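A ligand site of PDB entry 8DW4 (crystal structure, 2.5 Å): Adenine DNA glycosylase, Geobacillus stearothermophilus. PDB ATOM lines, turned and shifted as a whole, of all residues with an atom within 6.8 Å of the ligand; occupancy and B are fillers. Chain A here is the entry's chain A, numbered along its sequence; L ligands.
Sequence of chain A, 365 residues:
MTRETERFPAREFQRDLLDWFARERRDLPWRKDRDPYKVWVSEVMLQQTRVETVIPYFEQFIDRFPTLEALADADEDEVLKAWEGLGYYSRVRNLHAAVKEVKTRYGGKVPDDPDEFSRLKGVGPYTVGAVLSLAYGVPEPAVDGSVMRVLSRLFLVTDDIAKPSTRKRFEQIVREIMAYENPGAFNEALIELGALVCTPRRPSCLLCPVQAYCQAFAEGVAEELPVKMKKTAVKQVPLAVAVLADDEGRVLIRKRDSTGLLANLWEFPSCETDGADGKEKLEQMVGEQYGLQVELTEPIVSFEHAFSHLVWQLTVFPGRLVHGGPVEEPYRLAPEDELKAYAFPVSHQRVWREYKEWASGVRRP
SG of Cys 208 binds FE1 of the ligand (2.2 Å).
SG of Cys 214 binds FE4 of the ligand (2.2 Å).
The side-chain sulfur (SG) of Cys 205 is bound to an iron atom (FE2) of the ligand, 2.3 Å away.
SG of Cys 198 is bound to FE3 of the ligand.
The side-chain sulfur (SG) of Cys 208 sits close to the backbone NH (N) of Val 210.
SG of Cys 214 sits close to O of Arg 153, 3.2 Å away.
The backbone carbonyl oxygen (O) of Cys 205 sits close to the side-chain amide oxygen (OE1) of Gln 211 (3.1 Å).
The backbone carbonyl oxygen (O) of Cys 198 is in hydrogen-bond range of the guanidinium group (NH1) of Arg 153 (3.5 Å).
The backbone carbonyl oxygen (O) of Cys 198 sits at hydrogen-bond distance from the guanidinium group (NE) of Arg 149.
The backbone carbonyl oxygen (O) of Arg 153 lies within hydrogen-bond range of the backbone NH (N) of Ala 216 (2.9 Å).
The backbone carbonyl oxygen (O) of Thr 199 lies within hydrogen-bond range of the guanidinium group (NH1) of Arg 153 (2.9 Å).
O of Leu 154 sits at hydrogen-bond distance from N of Gln 215 (3.1 Å).
Merely in contact with the ligand: Ala 222 (3.3 Å), Arg 153 (3.6 Å), Gln 211 (3.6 Å), Phe 217 (3.8 Å) and Leu 154 (3.9 Å).
Hydrophobic or aromatic side chains within 4 Å of the ligand: Leu 154, Phe 217 and Ala 222.
Within 4 Å of the ligand: Arg 153, Leu 154, Cys 198, Cys 205, Cys 208, Gln 211, Cys 214, Phe 217 and Ala 222.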
ATOM      1  N   PHE A  13     -22.051 -14.079  -6.922  1.00  0.00           N
ATOM      2  CA  PHE A  13     -22.950 -13.440  -5.960  1.00  0.00           C
ATOM      3  C   PHE A  13     -24.182 -14.304  -5.707  1.00  0.00           C
ATOM      4  O   PHE A  13     -24.575 -14.510  -4.556  1.00  0.00           O
ATOM      5  CB  PHE A  13     -23.336 -12.050  -6.476  1.00  0.00           C
ATOM      6  CG  PHE A  13     -24.524 -11.437  -5.783  1.00  0.00           C
ATOM      7  CD1 PHE A  13     -25.811 -11.707  -6.223  1.00  0.00           C
ATOM      8  CD2 PHE A  13     -24.347 -10.567  -4.724  1.00  0.00           C
ATOM      9  CE1 PHE A  13     -26.902 -11.137  -5.602  1.00  0.00           C
ATOM     10  CE2 PHE A  13     -25.441 -10.001  -4.089  1.00  0.00           C
ATOM     11  CZ  PHE A  13     -26.719 -10.283  -4.531  1.00  0.00           C
ATOM     12  N   ARG A 149     -32.321  -0.934   0.084  1.00  0.00           N
ATOM     13  CA  ARG A 149     -31.131  -0.670   0.893  1.00  0.00           C
ATOM     14  C   ARG A 149     -29.999  -1.632   0.528  1.00  0.00           C
ATOM     15  O   ARG A 149     -28.848  -1.221   0.410  1.00  0.00           O
ATOM     16  CB  ARG A 149     -31.449  -0.773   2.385  1.00  0.00           C
ATOM     17  CG  ARG A 149     -30.210  -0.747   3.271  1.00  0.00           C
ATOM     18  CD  ARG A 149     -30.543  -0.737   4.746  1.00  0.00           C
ATOM     19  NE  ARG A 149     -30.953  -2.056   5.233  1.00  0.00           N
ATOM     20  CZ  ARG A 149     -32.213  -2.457   5.368  1.00  0.00           C
ATOM     21  NH1 ARG A 149     -33.238  -1.668   5.053  1.00  0.00           N
ATOM     22  NH2 ARG A 149     -32.467  -3.677   5.822  1.00  0.00           N
ATOM     23  N   VAL A 150     -30.327  -2.914   0.350  1.00  0.00           N
ATOM     24  CA  VAL A 150     -29.310  -3.894   0.001  1.00  0.00           C
ATOM     25  C   VAL A 150     -28.687  -3.546  -1.354  1.00  0.00           C
ATOM     26  O   VAL A 150     -27.458  -3.506  -1.499  1.00  0.00           O
ATOM     27  CB  VAL A 150     -29.911  -5.308  -0.007  1.00  0.00           C
ATOM     28  CG1 VAL A 150     -29.125  -6.231  -0.943  1.00  0.00           C
ATOM     29  CG2 VAL A 150     -29.931  -5.875   1.398  1.00  0.00           C
ATOM     30  N   ARG A 153     -26.382  -0.552  -1.563  1.00  0.00           N
ATOM     31  CA  ARG A 153     -25.063  -0.811  -1.007  1.00  0.00           C
ATOM     32  C   ARG A 153     -24.231  -1.739  -1.885  1.00  0.00           C
ATOM     33  O   ARG A 153     -23.035  -1.511  -2.060  1.00  0.00           O
ATOM     34  CB  ARG A 153     -25.191  -1.398   0.393  1.00  0.00           C
ATOM     35  CG  ARG A 153     -25.639  -0.391   1.443  1.00  0.00           C
ATOM     36  CD  ARG A 153     -26.195  -1.101   2.667  1.00  0.00           C
ATOM     37  NE  ARG A 153     -26.424  -0.193   3.789  1.00  0.00           N
ATOM     38  CZ  ARG A 153     -26.823  -0.574   4.990  1.00  0.00           C
ATOM     39  NH1 ARG A 153     -27.062  -1.847   5.263  1.00  0.00           N
ATOM     40  NH2 ARG A 153     -27.000   0.339   5.936  1.00  0.00           N
ATOM     41  N   LEU A 154     -24.852  -2.793  -2.429  1.00  0.00           N
ATOM     42  CA  LEU A 154     -24.126  -3.675  -3.333  1.00  0.00           C
ATOM     43  C   LEU A 154     -23.621  -2.937  -4.564  1.00  0.00           C
ATOM     44  O   LEU A 154     -22.574  -3.293  -5.106  1.00  0.00           O
ATOM     45  CB  LEU A 154     -25.033  -4.836  -3.754  1.00  0.00           C
ATOM     46  CG  LEU A 154     -25.267  -5.944  -2.714  1.00  0.00           C
ATOM     47  CD1 LEU A 154     -26.434  -6.825  -3.121  1.00  0.00           C
ATOM     48  CD2 LEU A 154     -24.012  -6.791  -2.521  1.00  0.00           C
ATOM     49  N   LEU A 193     -31.584 -11.352   3.556  1.00  0.00           N
ATOM     50  CA  LEU A 193     -30.307 -10.689   3.759  1.00  0.00           C
ATOM     51  C   LEU A 193     -30.509  -9.294   4.334  1.00  0.00           C
ATOM     52  O   LEU A 193     -29.798  -8.880   5.268  1.00  0.00           O
ATOM     53  CB  LEU A 193     -29.532 -10.615   2.450  1.00  0.00           C
ATOM     54  CG  LEU A 193     -28.084 -10.133   2.570  1.00  0.00           C
ATOM     55  CD1 LEU A 193     -27.211 -11.166   3.279  1.00  0.00           C
ATOM     56  CD2 LEU A 193     -27.497  -9.797   1.200  1.00  0.00           C
ATOM     57  N   VAL A 197     -28.746  -9.332   7.847  1.00  0.00           N
ATOM     58  CA  VAL A 197     -27.327  -9.034   7.671  1.00  0.00           C
ATOM     59  C   VAL A 197     -27.118  -7.570   7.319  1.00  0.00           C
ATOM     60  O   VAL A 197     -26.487  -6.821   8.079  1.00  0.00           O
ATOM     61  CB  VAL A 197     -26.719  -9.945   6.580  1.00  0.00           C
ATOM     62  CG1 VAL A 197     -25.252  -9.611   6.377  1.00  0.00           C
ATOM     63  CG2 VAL A 197     -26.903 -11.410   6.935  1.00  0.00           C
ATOM     64  N   CYS A 198     -27.639  -7.156   6.172  1.00  0.00           N
ATOM     65  CA  CYS A 198     -27.501  -5.779   5.706  1.00  0.00           C
ATOM     66  C   CYS A 198     -28.506  -4.888   6.432  1.00  0.00           C
ATOM     67  O   CYS A 198     -29.419  -4.304   5.842  1.00  0.00           O
ATOM     68  CB  CYS A 198     -27.677  -5.708   4.194  1.00  0.00           C
ATOM     69  SG  CYS A 198     -27.333  -4.083   3.468  1.00  0.00           S
ATOM     70  N   THR A 199     -28.317  -4.796   7.738  1.00  0.00           N
ATOM     71  CA  THR A 199     -29.297  -4.167   8.591  1.00  0.00           C
ATOM     72  C   THR A 199     -29.318  -2.658   8.343  1.00  0.00           C
ATOM     73  O   THR A 199     -28.337  -2.085   7.867  1.00  0.00           O
ATOM     74  CB  THR A 199     -28.991  -4.470  10.061  1.00  0.00           C
ATOM     75  OG1 THR A 199     -27.693  -3.970  10.400  1.00  0.00           O
ATOM     76  CG2 THR A 199     -29.043  -5.974  10.299  1.00  0.00           C
ATOM     77  N   PRO A 203     -24.647  -2.363   9.895  1.00  0.00           N
ATOM     78  CA  PRO A 203     -24.645  -3.593   9.084  1.00  0.00           C
ATOM     79  C   PRO A 203     -23.453  -4.477   9.398  1.00  0.00           C
ATOM     80  O   PRO A 203     -22.332  -4.010   9.593  1.00  0.00           O
ATOM     81  CB  PRO A 203     -24.592  -3.057   7.638  1.00  0.00           C
ATOM     82  CG  PRO A 203     -24.092  -1.652   7.755  1.00  0.00           C
ATOM     83  CD  PRO A 203     -24.589  -1.149   9.064  1.00  0.00           C
ATOM     84  N   SER A 204     -23.706  -5.789   9.437  1.00  0.00           N
ATOM     85  CA  SER A 204     -22.671  -6.777   9.760  1.00  0.00           C
ATOM     86  C   SER A 204     -22.088  -7.300   8.450  1.00  0.00           C
ATOM     87  O   SER A 204     -22.390  -8.394   7.971  1.00  0.00           O
ATOM     88  CB  SER A 204     -23.264  -7.893  10.606  1.00  0.00           C
ATOM     89  OG  SER A 204     -23.994  -7.379  11.700  1.00  0.00           O
ATOM     90  N   CYS A 205     -21.212  -6.476   7.856  1.00  0.00           N
ATOM     91  CA  CYS A 205     -20.662  -6.765   6.544  1.00  0.00           C
ATOM     92  C   CYS A 205     -19.584  -7.838   6.578  1.00  0.00           C
ATOM     93  O   CYS A 205     -19.262  -8.398   5.524  1.00  0.00           O
ATOM     94  CB  CYS A 205     -20.095  -5.482   5.930  1.00  0.00           C
ATOM     95  SG  CYS A 205     -21.230  -4.073   5.969  1.00  0.00           S
ATOM     96  N   LEU A 206     -19.011  -8.128   7.743  1.00  0.00           N
ATOM     97  CA  LEU A 206     -18.018  -9.191   7.834  1.00  0.00           C
ATOM     98  C   LEU A 206     -18.668 -10.563   7.748  1.00  0.00           C
ATOM     99  O   LEU A 206     -18.047 -11.516   7.253  1.00  0.00           O
ATOM    100  CB  LEU A 206     -17.237  -9.059   9.140  1.00  0.00           C
ATOM    101  CG  LEU A 206     -16.528  -7.714   9.367  1.00  0.00           C
ATOM    102  CD1 LEU A 206     -15.842  -7.687  10.720  1.00  0.00           C
ATOM    103  CD2 LEU A 206     -15.531  -7.423   8.250  1.00  0.00           C
ATOM    104  N   LEU A 207     -19.911 -10.685   8.224  1.00  0.00           N
ATOM    105  CA  LEU A 207     -20.691 -11.903   8.131  1.00  0.00           C
ATOM    106  C   LEU A 207     -21.435 -12.024   6.804  1.00  0.00           C
ATOM    107  O   LEU A 207     -22.093 -13.052   6.572  1.00  0.00           O
ATOM    108  CB  LEU A 207     -21.686 -11.960   9.295  1.00  0.00           C
ATOM    109  CG  LEU A 207     -21.065 -11.966  10.689  1.00  0.00           C
ATOM    110  CD1 LEU A 207     -21.962 -11.315  11.736  1.00  0.00           C
ATOM    111  CD2 LEU A 207     -20.726 -13.386  11.101  1.00  0.00           C
ATOM    112  N   CYS A 208     -21.355 -11.014   5.952  1.00  0.00           N
ATOM    113  CA  CYS A 208     -22.167 -10.971   4.755  1.00  0.00           C
ATOM    114  C   CYS A 208     -21.672 -11.985   3.724  1.00  0.00           C
ATOM    115  O   CYS A 208     -20.475 -12.017   3.429  1.00  0.00           O
ATOM    116  CB  CYS A 208     -22.147  -9.559   4.170  1.00  0.00           C
ATOM    117  SG  CYS A 208     -23.251  -9.287   2.762  1.00  0.00           S
ATOM    118  N   PRO A 209     -22.548 -12.826   3.155  1.00  0.00           N
ATOM    119  CA  PRO A 209     -22.101 -13.758   2.117  1.00  0.00           C
ATOM    120  C   PRO A 209     -21.607 -13.080   0.846  1.00  0.00           C
ATOM    121  O   PRO A 209     -20.974 -13.746   0.015  1.00  0.00           O
ATOM    122  CB  PRO A 209     -23.343 -14.598   1.836  1.00  0.00           C
ATOM    123  CG  PRO A 209     -24.476 -13.686   2.187  1.00  0.00           C
ATOM    124  CD  PRO A 209     -24.001 -12.943   3.396  1.00  0.00           C
ATOM    125  N   VAL A 210     -21.890 -11.791   0.666  1.00  0.00           N
ATOM    126  CA  VAL A 210     -21.596 -11.111  -0.590  1.00  0.00           C
ATOM    127  C   VAL A 210     -20.774  -9.852  -0.324  1.00  0.00           C
ATOM    128  O   VAL A 210     -20.897  -8.854  -1.039  1.00  0.00           O
ATOM    129  CB  VAL A 210     -22.906 -10.771  -1.337  1.00  0.00           C
ATOM    130  CG1 VAL A 210     -23.564 -12.058  -1.808  1.00  0.00           C
ATOM    131  CG2 VAL A 210     -23.868  -9.990  -0.450  1.00  0.00           C
ATOM    132  N   GLN A 211     -19.916  -9.904   0.700  1.00  0.00           N
ATOM    133  CA  GLN A 211     -19.096  -8.736   1.037  1.00  0.00           C
ATOM    134  C   GLN A 211     -18.161  -8.370  -0.106  1.00  0.00           C
ATOM    135  O   GLN A 211     -17.940  -7.185  -0.382  1.00  0.00           O
ATOM    136  CB  GLN A 211     -18.307  -8.990   2.331  1.00  0.00           C
ATOM    137  CG  GLN A 211     -17.073  -9.886   2.175  1.00  0.00           C
ATOM    138  CD  GLN A 211     -16.197  -9.876   3.411  1.00  0.00           C
ATOM    139  OE1 GLN A 211     -16.447  -9.123   4.356  1.00  0.00           O
ATOM    140  NE2 GLN A 211     -15.159 -10.705   3.407  1.00  0.00           N
ATOM    141  N   ALA A 212     -17.589  -9.378  -0.769  1.00  0.00           N
ATOM    142  CA  ALA A 212     -16.647  -9.095  -1.852  1.00  0.00           C
ATOM    143  C   ALA A 212     -17.328  -8.358  -2.996  1.00  0.00           C
ATOM    144  O   ALA A 212     -16.752  -7.443  -3.580  1.00  0.00           O
ATOM    145  CB  ALA A 212     -16.029 -10.401  -2.344  1.00  0.00           C
ATOM    146  N   TYR A 213     -18.558  -8.740  -3.317  1.00  0.00           N
ATOM    147  CA  TYR A 213     -19.273  -8.204  -4.466  1.00  0.00           C
ATOM    148  C   TYR A 213     -19.986  -6.888  -4.155  1.00  0.00           C
ATOM    149  O   TYR A 213     -20.829  -6.464  -4.939  1.00  0.00           O
ATOM    150  CB  TYR A 213     -20.285  -9.231  -4.971  1.00  0.00           C
ATOM    151  CG  TYR A 213     -19.796 -10.657  -4.797  1.00  0.00           C
ATOM    152  CD1 TYR A 213     -18.655 -11.096  -5.443  1.00  0.00           C
ATOM    153  CD2 TYR A 213     -20.473 -11.558  -3.987  1.00  0.00           C
ATOM    154  CE1 TYR A 213     -18.192 -12.391  -5.290  1.00  0.00           C
ATOM    155  CE2 TYR A 213     -20.028 -12.850  -3.821  1.00  0.00           C
ATOM    156  CZ  TYR A 213     -18.885 -13.268  -4.476  1.00  0.00           C
ATOM    157  OH  TYR A 213     -18.427 -14.559  -4.315  1.00  0.00           O
ATOM    158  N   CYS A 214     -19.642  -6.241  -3.042  1.00  0.00           N
ATOM    159  CA  CYS A 214     -20.377  -5.082  -2.546  1.00  0.00           C
ATOM    160  C   CYS A 214     -19.506  -3.841  -2.641  1.00  0.00           C
ATOM    161  O   CYS A 214     -18.471  -3.735  -1.963  1.00  0.00           O
ATOM    162  CB  CYS A 214     -20.818  -5.318  -1.099  1.00  0.00           C
ATOM    163  SG  CYS A 214     -21.902  -4.023  -0.441  1.00  0.00           S
ATOM    164  N   GLN A 215     -19.932  -2.887  -3.469  1.00  0.00           N
ATOM    165  CA  GLN A 215     -19.181  -1.656  -3.672  1.00  0.00           C
ATOM    166  C   GLN A 215     -19.169  -0.791  -2.416  1.00  0.00           C
ATOM    167  O   GLN A 215     -18.146  -0.171  -2.091  1.00  0.00           O
ATOM    168  CB  GLN A 215     -19.746  -0.886  -4.864  1.00  0.00           C
ATOM    169  CG  GLN A 215     -19.674  -1.660  -6.180  1.00  0.00           C
ATOM    170  CD  GLN A 215     -20.445  -1.001  -7.313  1.00  0.00           C
ATOM    171  OE1 GLN A 215     -21.046  -1.686  -8.140  1.00  0.00           O
ATOM    172  NE2 GLN A 215     -20.416   0.326  -7.357  1.00  0.00           N
ATOM    173  N   ALA A 216     -20.294  -0.729  -1.704  1.00  0.00           N
ATOM    174  CA  ALA A 216     -20.392   0.165  -0.545  1.00  0.00           C
ATOM    175  C   ALA A 216     -19.442  -0.260   0.564  1.00  0.00           C
ATOM    176  O   ALA A 216     -18.811   0.586   1.210  1.00  0.00           O
ATOM    177  CB  ALA A 216     -21.831   0.207  -0.032  1.00  0.00           C
ATOM    178  N   PHE A 217     -19.343  -1.563   0.818  1.00  0.00           N
ATOM    179  CA  PHE A 217     -18.423  -2.054   1.839  1.00  0.00           C
ATOM    180  C   PHE A 217     -16.975  -1.746   1.471  1.00  0.00           C
ATOM    181  O   PHE A 217     -16.193  -1.274   2.290  1.00  0.00           O
ATOM    182  CB  PHE A 217     -18.641  -3.550   2.048  1.00  0.00           C
ATOM    183  CG  PHE A 217     -17.576  -4.234   2.862  1.00  0.00           C
ATOM    184  CD1 PHE A 217     -17.190  -3.734   4.090  1.00  0.00           C
ATOM    185  CD2 PHE A 217     -16.995  -5.398   2.402  1.00  0.00           C
ATOM    186  CE1 PHE A 217     -16.217  -4.373   4.836  1.00  0.00           C
ATOM    187  CE2 PHE A 217     -16.025  -6.047   3.138  1.00  0.00           C
ATOM    188  CZ  PHE A 217     -15.642  -5.538   4.361  1.00  0.00           C
ATOM    189  N   ALA A 218     -16.618  -2.025   0.215  1.00  0.00           N
ATOM    190  CA  ALA A 218     -15.310  -1.632  -0.298  1.00  0.00           C
ATOM    191  C   ALA A 218     -14.999  -0.169   0.007  1.00  0.00           C
ATOM    192  O   ALA A 218     -13.951   0.154   0.567  1.00  0.00           O
ATOM    193  CB  ALA A 218     -15.245  -1.882  -1.802  1.00  0.00           C
ATOM    194  N   VAL A 221     -18.840   2.864   3.157  1.00  0.00           N
ATOM    195  CA  VAL A 221     -19.939   3.815   3.317  1.00  0.00           C
ATOM    196  C   VAL A 221     -21.280   3.112   3.404  1.00  0.00           C
ATOM    197  O   VAL A 221     -22.337   3.745   3.228  1.00  0.00           O
ATOM    198  CB  VAL A 221     -19.920   4.835   2.164  1.00  0.00           C
ATOM    199  CG1 VAL A 221     -18.744   5.778   2.337  1.00  0.00           C
ATOM    200  CG2 VAL A 221     -19.853   4.121   0.826  1.00  0.00           C
ATOM    201  N   ALA A 222     -21.273   1.813   3.676  1.00  0.00           N
ATOM    202  CA  ALA A 222     -22.533   1.085   3.827  1.00  0.00           C
ATOM    203  C   ALA A 222     -23.372   1.684   4.951  1.00  0.00           C
ATOM    204  O   ALA A 222     -24.605   1.723   4.873  1.00  0.00           O
ATOM    205  CB  ALA A 222     -22.268  -0.392   4.081  1.00  0.00           C
ATOM    206  N   GLU A 223     -22.719   2.165   6.020  1.00  0.00           N
ATOM    207  CA  GLU A 223     -23.431   2.812   7.107  1.00  0.00           C
ATOM    208  C   GLU A 223     -24.036   4.149   6.701  1.00  0.00           C
ATOM    209  O   GLU A 223     -24.828   4.714   7.460  1.00  0.00           O
ATOM    210  CB  GLU A 223     -22.481   3.024   8.296  1.00  0.00           C
HETATM  211 FE1  LIG L   1     -23.292  -7.142   3.019  1.00  0.00          FE
HETATM  212 FE2  LIG L   1     -22.269  -4.855   4.108  1.00  0.00          FE
HETATM  213 FE3  LIG L   1     -24.808  -4.872   3.105  1.00  0.00          FE
HETATM  214 FE4  LIG L   1     -22.672  -5.016   1.417  1.00  0.00          FE
HETATM  215  S1  LIG L   1     -23.225  -3.276   2.778  1.00  0.00           S
HETATM  216  S2  LIG L   1     -24.560  -6.281   1.329  1.00  0.00           S
HETATM  217  S3  LIG L   1     -21.220  -6.253   2.657  1.00  0.00           S
HETATM  218  S4  LIG L   1     -24.031  -6.062   4.881  1.00  0.00           S
